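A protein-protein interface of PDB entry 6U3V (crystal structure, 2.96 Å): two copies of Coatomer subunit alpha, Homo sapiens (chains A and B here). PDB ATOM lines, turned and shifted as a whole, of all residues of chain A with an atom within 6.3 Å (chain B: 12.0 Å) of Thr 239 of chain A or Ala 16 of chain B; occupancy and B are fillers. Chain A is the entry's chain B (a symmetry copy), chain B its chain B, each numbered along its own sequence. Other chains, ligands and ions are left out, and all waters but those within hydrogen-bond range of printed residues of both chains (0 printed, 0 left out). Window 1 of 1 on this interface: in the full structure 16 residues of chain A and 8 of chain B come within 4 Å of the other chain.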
ATOM      1  N   GLU A 199       7.893   6.241  -0.647  1.00  0.00           N
ATOM      2  CA  GLU A 199       8.614   6.824   0.479  1.00  0.00           C
ATOM      3  C   GLU A 199      10.005   7.287   0.057  1.00  0.00           C
ATOM      4  O   GLU A 199      10.431   8.387   0.424  1.00  0.00           O
ATOM      5  CB  GLU A 199       8.676   5.822   1.631  1.00  0.00           C
ATOM      6  CG  GLU A 199       9.636   6.158   2.762  1.00  0.00           C
ATOM      7  CD  GLU A 199       9.061   7.088   3.825  1.00  0.00           C
ATOM      8  OE1 GLU A 199       8.091   7.842   3.549  1.00  0.00           O
ATOM      9  OE2 GLU A 199       9.606   7.063   4.953  1.00  0.00           O
ATOM     10  N   ARG A 202       9.577  10.482  -1.755  1.00  0.00           N
ATOM     11  CA  ARG A 202       9.217  11.570  -0.855  1.00  0.00           C
ATOM     12  C   ARG A 202      10.464  12.139  -0.181  1.00  0.00           C
ATOM     13  O   ARG A 202      10.602  13.363  -0.036  1.00  0.00           O
ATOM     14  CB  ARG A 202       8.170  11.071   0.146  1.00  0.00           C
ATOM     15  CG  ARG A 202       7.732  12.058   1.204  1.00  0.00           C
ATOM     16  CD  ARG A 202       7.034  11.328   2.341  1.00  0.00           C
ATOM     17  NE  ARG A 202       7.999  10.745   3.273  1.00  0.00           N
ATOM     18  CZ  ARG A 202       8.767  11.432   4.111  1.00  0.00           C
ATOM     19  NH1 ARG A 202       8.684  12.755   4.180  1.00  0.00           N
ATOM     20  NH2 ARG A 202       9.619  10.786   4.893  1.00  0.00           N
ATOM     21  N   ALA A 220       3.013  10.966   1.562  1.00  0.00           N
ATOM     22  CA  ALA A 220       2.938  10.250   2.829  1.00  0.00           C
ATOM     23  C   ALA A 220       1.540   9.681   3.049  1.00  0.00           C
ATOM     24  O   ALA A 220       1.396   8.580   3.588  1.00  0.00           O
ATOM     25  CB  ALA A 220       3.352  11.162   3.982  1.00  0.00           C
ATOM     26  N   ILE A 234       1.918   0.886  10.842  1.00  0.00           N
ATOM     27  CA  ILE A 234       2.070   1.799  11.970  1.00  0.00           C
ATOM     28  C   ILE A 234       3.156   2.830  11.679  1.00  0.00           C
ATOM     29  O   ILE A 234       2.968   4.027  11.903  1.00  0.00           O
ATOM     30  CB  ILE A 234       2.355   1.014  13.254  1.00  0.00           C
ATOM     31  CG1 ILE A 234       1.113   0.202  13.611  1.00  0.00           C
ATOM     32  CG2 ILE A 234       2.713   1.959  14.374  1.00  0.00           C
ATOM     33  CD1 ILE A 234       1.205  -0.498  14.913  1.00  0.00           C
ATOM     34  N   LEU A 235       4.284   2.389  11.122  1.00  0.00           N
ATOM     35  CA  LEU A 235       5.363   3.312  10.782  1.00  0.00           C
ATOM     36  C   LEU A 235       4.932   4.316   9.715  1.00  0.00           C
ATOM     37  O   LEU A 235       5.321   5.489   9.774  1.00  0.00           O
ATOM     38  CB  LEU A 235       6.605   2.526  10.339  1.00  0.00           C
ATOM     39  CG  LEU A 235       7.269   1.685  11.448  1.00  0.00           C
ATOM     40  CD1 LEU A 235       8.275   0.731  10.904  1.00  0.00           C
ATOM     41  CD2 LEU A 235       7.954   2.592  12.455  1.00  0.00           C
ATOM     42  N   VAL A 236       4.136   3.888   8.731  1.00  0.00           N
ATOM     43  CA  VAL A 236       3.776   4.848   7.695  1.00  0.00           C
ATOM     44  C   VAL A 236       2.702   5.802   8.198  1.00  0.00           C
ATOM     45  O   VAL A 236       2.657   6.956   7.759  1.00  0.00           O
ATOM     46  CB  VAL A 236       3.344   4.180   6.371  1.00  0.00           C
ATOM     47  CG1 VAL A 236       4.062   2.877   6.146  1.00  0.00           C
ATOM     48  CG2 VAL A 236       1.824   4.046   6.243  1.00  0.00           C
ATOM     49  N   LEU A 237       1.837   5.355   9.119  1.00  0.00           N
ATOM     50  CA  LEU A 237       0.884   6.273   9.738  1.00  0.00           C
ATOM     51  C   LEU A 237       1.588   7.256  10.664  1.00  0.00           C
ATOM     52  O   LEU A 237       1.250   8.444  10.688  1.00  0.00           O
ATOM     53  CB  LEU A 237      -0.183   5.491  10.488  1.00  0.00           C
ATOM     54  CG  LEU A 237      -1.255   4.891   9.599  1.00  0.00           C
ATOM     55  CD1 LEU A 237      -2.107   3.912  10.367  1.00  0.00           C
ATOM     56  CD2 LEU A 237      -2.094   6.002   9.041  1.00  0.00           C
ATOM     57  N   ARG A 238       2.572   6.790  11.432  1.00  0.00           N
ATOM     58  CA  ARG A 238       3.410   7.718  12.188  1.00  0.00           C
ATOM     59  C   ARG A 238       4.020   8.775  11.278  1.00  0.00           C
ATOM     60  O   ARG A 238       3.999   9.963  11.599  1.00  0.00           O
ATOM     61  CB  ARG A 238       4.506   6.951  12.928  1.00  0.00           C
ATOM     62  CG  ARG A 238       4.109   6.376  14.250  1.00  0.00           C
ATOM     63  CD  ARG A 238       5.183   5.429  14.738  1.00  0.00           C
ATOM     64  NE  ARG A 238       6.490   6.060  14.818  1.00  0.00           N
ATOM     65  CZ  ARG A 238       7.575   5.468  15.297  1.00  0.00           C
ATOM     66  NH1 ARG A 238       7.517   4.222  15.764  1.00  0.00           N
ATOM     67  NH2 ARG A 238       8.725   6.122  15.304  1.00  0.00           N
ATOM     68  N   THR A 239       4.562   8.365  10.127  1.00  0.00           N
ATOM     69  CA  THR A 239       5.134   9.348   9.211  1.00  0.00           C
ATOM     70  C   THR A 239       4.059  10.322   8.728  1.00  0.00           C
ATOM     71  O   THR A 239       4.250  11.544   8.759  1.00  0.00           O
ATOM     72  CB  THR A 239       5.821   8.653   8.030  1.00  0.00           C
ATOM     73  OG1 THR A 239       6.841   7.774   8.509  1.00  0.00           O
ATOM     74  CG2 THR A 239       6.495   9.664   7.141  1.00  0.00           C
ATOM     75  N   ALA A 240       2.905   9.802   8.296  1.00  0.00           N
ATOM     76  CA  ALA A 240       1.839  10.682   7.822  1.00  0.00           C
ATOM     77  C   ALA A 240       1.333  11.587   8.930  1.00  0.00           C
ATOM     78  O   ALA A 240       0.963  12.732   8.670  1.00  0.00           O
ATOM     79  CB  ALA A 240       0.682   9.870   7.240  1.00  0.00           C
ATOM     80  N   LEU A 241       1.322  11.098  10.170  1.00  0.00           N
ATOM     81  CA  LEU A 241       0.827  11.900  11.282  1.00  0.00           C
ATOM     82  C   LEU A 241       1.732  13.101  11.554  1.00  0.00           C
ATOM     83  O   LEU A 241       1.224  14.198  11.816  1.00  0.00           O
ATOM     84  CB  LEU A 241       0.659  11.029  12.525  1.00  0.00           C
ATOM     85  CG  LEU A 241       0.131  11.728  13.775  1.00  0.00           C
ATOM     86  CD1 LEU A 241      -1.051  12.564  13.400  1.00  0.00           C
ATOM     87  CD2 LEU A 241      -0.300  10.693  14.759  1.00  0.00           C
ATOM     88  N   ASN A 242       3.069  12.923  11.525  1.00  0.00           N
ATOM     89  CA  ASN A 242       3.968  14.073  11.678  1.00  0.00           C
ATOM     90  C   ASN A 242       3.758  15.090  10.584  1.00  0.00           C
ATOM     91  O   ASN A 242       3.524  16.274  10.861  1.00  0.00           O
ATOM     92  CB  ASN A 242       5.440  13.685  11.625  1.00  0.00           C
ATOM     93  CG  ASN A 242       5.987  13.300  12.938  1.00  0.00           C
ATOM     94  OD1 ASN A 242       5.252  13.151  13.913  1.00  0.00           O
ATOM     95  ND2 ASN A 242       7.311  13.207  13.008  1.00  0.00           N
ATOM     96  N   LEU A 243       3.835  14.642   9.326  1.00  0.00           N
ATOM     97  CA  LEU A 243       3.848  15.600   8.234  1.00  0.00           C
ATOM     98  C   LEU A 243       2.549  16.396   8.182  1.00  0.00           C
ATOM     99  O   LEU A 243       2.576  17.622   8.005  1.00  0.00           O
ATOM    100  CB  LEU A 243       4.138  14.878   6.928  1.00  0.00           C
ATOM    101  CG  LEU A 243       5.564  14.303   6.966  1.00  0.00           C
ATOM    102  CD1 LEU A 243       5.883  13.525   5.728  1.00  0.00           C
ATOM    103  CD2 LEU A 243       6.616  15.366   7.197  1.00  0.00           C
ATOM    104  N   PHE A 244       1.407  15.736   8.412  1.00  0.00           N
ATOM    105  CA  PHE A 244       0.139  16.461   8.438  1.00  0.00           C
ATOM    106  C   PHE A 244      -0.013  17.298   9.699  1.00  0.00           C
ATOM    107  O   PHE A 244      -0.744  18.296   9.690  1.00  0.00           O
ATOM    108  CB  PHE A 244      -1.042  15.506   8.279  1.00  0.00           C
ATOM    109  CG  PHE A 244      -1.365  15.171   6.836  1.00  0.00           C
ATOM    110  CD1 PHE A 244      -0.512  14.373   6.077  1.00  0.00           C
ATOM    111  CD2 PHE A 244      -2.522  15.658   6.236  1.00  0.00           C
ATOM    112  CE1 PHE A 244      -0.812  14.060   4.754  1.00  0.00           C
ATOM    113  CE2 PHE A 244      -2.830  15.349   4.906  1.00  0.00           C
ATOM    114  CZ  PHE A 244      -1.972  14.555   4.162  1.00  0.00           C
ATOM    115  N   LEU A 260      -3.851   4.691  13.354  1.00  0.00           N
ATOM    116  CA  LEU A 260      -2.632   4.182  13.960  1.00  0.00           C
ATOM    117  C   LEU A 260      -2.946   3.479  15.273  1.00  0.00           C
ATOM    118  O   LEU A 260      -2.456   2.377  15.534  1.00  0.00           O
ATOM    119  CB  LEU A 260      -1.678   5.343  14.202  1.00  0.00           C
ATOM    120  CG  LEU A 260      -0.225   5.083  14.544  1.00  0.00           C
ATOM    121  CD1 LEU A 260       0.546   6.377  14.314  1.00  0.00           C
ATOM    122  CD2 LEU A 260       0.020   4.532  15.914  1.00  0.00           C
ATOM    123  N   GLU B  10      18.853   7.536   5.464  1.00  0.00           N
ATOM    124  CA  GLU B  10      17.792   6.879   4.700  1.00  0.00           C
ATOM    125  C   GLU B  10      17.154   5.711   5.463  1.00  0.00           C
ATOM    126  O   GLU B  10      16.866   4.667   4.872  1.00  0.00           O
ATOM    127  CB  GLU B  10      18.328   6.382   3.353  1.00  0.00           C
ATOM    128  N   GLY B  11      16.940   5.894   6.771  1.00  0.00           N
ATOM    129  CA  GLY B  11      16.186   4.952   7.585  1.00  0.00           C
ATOM    130  C   GLY B  11      14.705   5.285   7.572  1.00  0.00           C
ATOM    131  O   GLY B  11      14.175   5.614   6.506  1.00  0.00           O
ATOM    132  N   TRP B  12      14.005   5.201   8.715  1.00  0.00           N
ATOM    133  CA  TRP B  12      12.675   5.812   8.754  1.00  0.00           C
ATOM    134  C   TRP B  12      12.778   7.305   9.049  1.00  0.00           C
ATOM    135  O   TRP B  12      11.953   8.090   8.560  1.00  0.00           O
ATOM    136  CB  TRP B  12      11.753   5.106   9.764  1.00  0.00           C
ATOM    137  CG  TRP B  12      11.192   3.781   9.243  1.00  0.00           C
ATOM    138  CD1 TRP B  12      11.719   2.534   9.449  1.00  0.00           C
ATOM    139  CD2 TRP B  12      10.021   3.578   8.423  1.00  0.00           C
ATOM    140  NE1 TRP B  12      10.957   1.579   8.815  1.00  0.00           N
ATOM    141  CE2 TRP B  12       9.915   2.193   8.176  1.00  0.00           C
ATOM    142  CE3 TRP B  12       9.060   4.427   7.876  1.00  0.00           C
ATOM    143  CZ2 TRP B  12       8.881   1.642   7.406  1.00  0.00           C
ATOM    144  CZ3 TRP B  12       8.034   3.868   7.109  1.00  0.00           C
ATOM    145  CH2 TRP B  12       7.961   2.495   6.880  1.00  0.00           C
ATOM    146  N   GLY B  13      13.798   7.710   9.820  1.00  0.00           N
ATOM    147  CA  GLY B  13      14.199   9.102   9.926  1.00  0.00           C
ATOM    148  C   GLY B  13      13.520   9.865  11.044  1.00  0.00           C
ATOM    149  O   GLY B  13      12.766   9.326  11.863  1.00  0.00           O
ATOM    150  N   GLU B  14      13.819  11.168  11.081  1.00  0.00           N
ATOM    151  CA  GLU B  14      13.100  12.077  11.967  1.00  0.00           C
ATOM    152  C   GLU B  14      11.710  12.408  11.437  1.00  0.00           C
ATOM    153  O   GLU B  14      10.900  12.986  12.174  1.00  0.00           O
ATOM    154  CB  GLU B  14      13.916  13.357  12.190  1.00  0.00           C
ATOM    155  N   ASP B  15      11.422  12.048  10.180  1.00  0.00           N
ATOM    156  CA  ASP B  15      10.083  12.134   9.608  1.00  0.00           C
ATOM    157  C   ASP B  15       9.122  11.122  10.221  1.00  0.00           C
ATOM    158  O   ASP B  15       7.910  11.229  10.008  1.00  0.00           O
ATOM    159  CB  ASP B  15      10.146  11.916   8.085  1.00  0.00           C
ATOM    160  CG  ASP B  15      10.780  13.088   7.332  1.00  0.00           C
ATOM    161  OD1 ASP B  15      10.366  14.250   7.559  1.00  0.00           O
ATOM    162  OD2 ASP B  15      11.686  12.836   6.503  1.00  0.00           O
ATOM    163  N   ALA B  16       9.626  10.135  10.957  1.00  0.00           N
ATOM    164  CA  ALA B  16       8.784   9.108  11.546  1.00  0.00           C
ATOM    165  C   ALA B  16       8.636   9.239  13.054  1.00  0.00           C
ATOM    166  O   ALA B  16       7.779   8.562  13.632  1.00  0.00           O
ATOM    167  CB  ALA B  16       9.331   7.712  11.214  1.00  0.00           C
ATOM    168  N   GLU B  17       9.439  10.085  13.701  1.00  0.00           N
ATOM    169  CA  GLU B  17       9.396  10.252  15.147  1.00  0.00           C
ATOM    170  C   GLU B  17       8.359  11.306  15.504  1.00  0.00           C
ATOM    171  O   GLU B  17       8.424  12.431  15.001  1.00  0.00           O
ATOM    172  CB  GLU B  17      10.763  10.672  15.690  1.00  0.00           C
ATOM    173  CG  GLU B  17      11.959  10.087  14.948  1.00  0.00           C
ATOM    174  CD  GLU B  17      12.524   8.864  15.631  1.00  0.00           C
ATOM    175  OE1 GLU B  17      12.144   8.610  16.796  1.00  0.00           O
ATOM    176  OE2 GLU B  17      13.346   8.161  14.997  1.00  0.00           O
ATOM    177  N   LEU B  18       7.420  10.949  16.380  1.00  0.00           N
ATOM    178  CA  LEU B  18       6.411  11.895  16.849  1.00  0.00           C
ATOM    179  C   LEU B  18       7.017  12.838  17.899  1.00  0.00           C
ATOM    180  O   LEU B  18       7.707  12.392  18.826  1.00  0.00           O
ATOM    181  CB  LEU B  18       5.201  11.134  17.406  1.00  0.00           C
ATOM    182  CG  LEU B  18       4.558  10.075  16.482  1.00  0.00           C
ATOM    183  CD1 LEU B  18       3.515   9.205  17.180  1.00  0.00           C
ATOM    184  CD2 LEU B  18       3.936  10.714  15.270  1.00  0.00           C
ATOM    185  N   GLN B  19       6.758  14.146  17.747  1.00  0.00           N
ATOM    186  CA  GLN B  19       7.487  15.206  18.432  1.00  0.00           C
ATOM    187  C   GLN B  19       6.668  15.786  19.581  1.00  0.00           C
ATOM    188  O   GLN B  19       5.546  15.358  19.862  1.00  0.00           O
ATOM    189  CB  GLN B  19       7.858  16.332  17.459  1.00  0.00           C
ATOM    190  CG  GLN B  19       8.636  15.911  16.218  1.00  0.00           C
ATOM    191  CD  GLN B  19      10.112  15.699  16.487  1.00  0.00           C
ATOM    192  OE1 GLN B  19      10.618  14.567  16.401  1.00  0.00           O
ATOM    193  NE2 GLN B  19      10.821  16.789  16.800  1.00  0.00           N
ATOM    194  N   LEU B  20       7.252  16.793  20.239  1.00  0.00           N
ATOM    195  CA  LEU B  20       6.542  17.579  21.249  1.00  0.00           C
ATOM    196  C   LEU B  20       5.469  18.445  20.591  1.00  0.00           C
ATOM    197  O   LEU B  20       5.777  19.210  19.665  1.00  0.00           O
ATOM    198  CB  LEU B  20       7.530  18.469  22.022  1.00  0.00           C
ATOM    199  CG  LEU B  20       8.192  19.710  21.379  1.00  0.00           C
ATOM    200  CD1 LEU B  20       7.460  21.015  21.678  1.00  0.00           C
ATOM    201  CD2 LEU B  20       9.638  19.836  21.797  1.00  0.00           C
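ND2 of Asn 242 of chain A sits at hydrogen-bond distance from O of Glu 17 of chain B (2.4 Å). NE of Arg 238 of chain A sits at hydrogen-bond distance from O of Ala 16 of chain B (3.1 Å). The side-chain carboxylate of Asp 15 of chain B lies within salt-bridge range of the guanidinium group of Arg 202 of chain A.
The side-chain amide oxygen (OE1) of Gln 19 of chain B lies close to the backbone carbonyl oxygen (O) of Glu 17 of chain B (3.4 Å). The side-chain carboxylate (OE1) of Glu 199 of chain A is in salt-bridge range of the guanidinium group (NE) of Arg 202 of chain A (2.9 Å). The side-chain hydroxyl of Thr 239 of chain A sits at hydrogen-bond distance from the backbone carbonyl oxygen of Leu 235 of chain A, at 3.0 Å.
Among the printed residues, pairs that only touch across the chains: Asn 242 of chain A with Leu 18 of chain B, Thr 239 of chain A with Asp 15 of chain B, Leu 235 of chain A with Trp 12 of chain B, Asn 242 of chain A with Asp 15 of chain B, Thr 239 of chain A with Ala 16 of chain B, Asn 242 of chain A with Glu 14 of chain B, Arg 238 of chain A with Leu 18 of chain B, Leu 243 of chain A with Asp 15 of chain B, Glu 199 of chain A with Trp 12 of chain B and Val 236 of chain A with Trp 12 of chain B.
Thr 239 of chain A touches just these residues of chain B: Asp 15 and Ala 16. Printed residues of chain A within 4 Å of Ala 16 of chain B: Arg 238 (3.1 Å) and Thr 239 (3.7 Å). Ala 220 of chain A touches none of the printed residues of chain B. Of chain B, only Trp 12 (3.5 Å) comes within 4 Å of Leu 235 of chain A. Ala 240 of chain A touches none of the printed residues of chain B. Of chain B, only Glu 14, Asp 15, Glu 17 and Leu 18 come within 4 Å of Asn 242 of chain A. Leu 243 of chain A touches one residue of chain B. Printed residues of chain A within 4 Å of Asp 15 of chain B: Arg 202 (3.3 Å), Thr 239 (3.4 Å), Asn 242 (3.6 Å) and Leu 243 (3.9 Å). Of the printed residues of chain A, Glu 17 of chain B touches Asn 242 (2.4 Å). Of the printed residues of chain A, Glu 14 of chain B touches Asn 242 (3.7 Å). Printed residues of chain B within 4 Å of Glu 199 of chain A: Trp 12. Of the printed residues of chain A, Leu 18 of chain B touches Arg 238 and Asn 242. Gly 11 of chain B touches none of the printed residues of chain A. The nearest residue of chain B that does not touch Thr 239 of chain A is Trp 12 of chain B (4.1 Å). The nearest residue of chain A that does not touch Ala 16 of chain B is Asn 242 of chain A (4.2 Å).
Hydrophobic or aromatic side chains of chain A that line the printed part of chain B: Leu 235, Val 236 and Leu 243. Along chain A the printed residues that touch a printed residue of chain B span positions 199 to 243. Among the printed residues, Asp or Glu carboxylates within 4 Å of a Lys or Arg side-chain nitrogen of the other chain: Arg 202 of chain A with Asp 15 of chain B (3.3 Å).
No position is printed for both chains. Of the 13 pairs that touch across the chains among the printed residues, none has its exchanged pair printed and touching as well.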
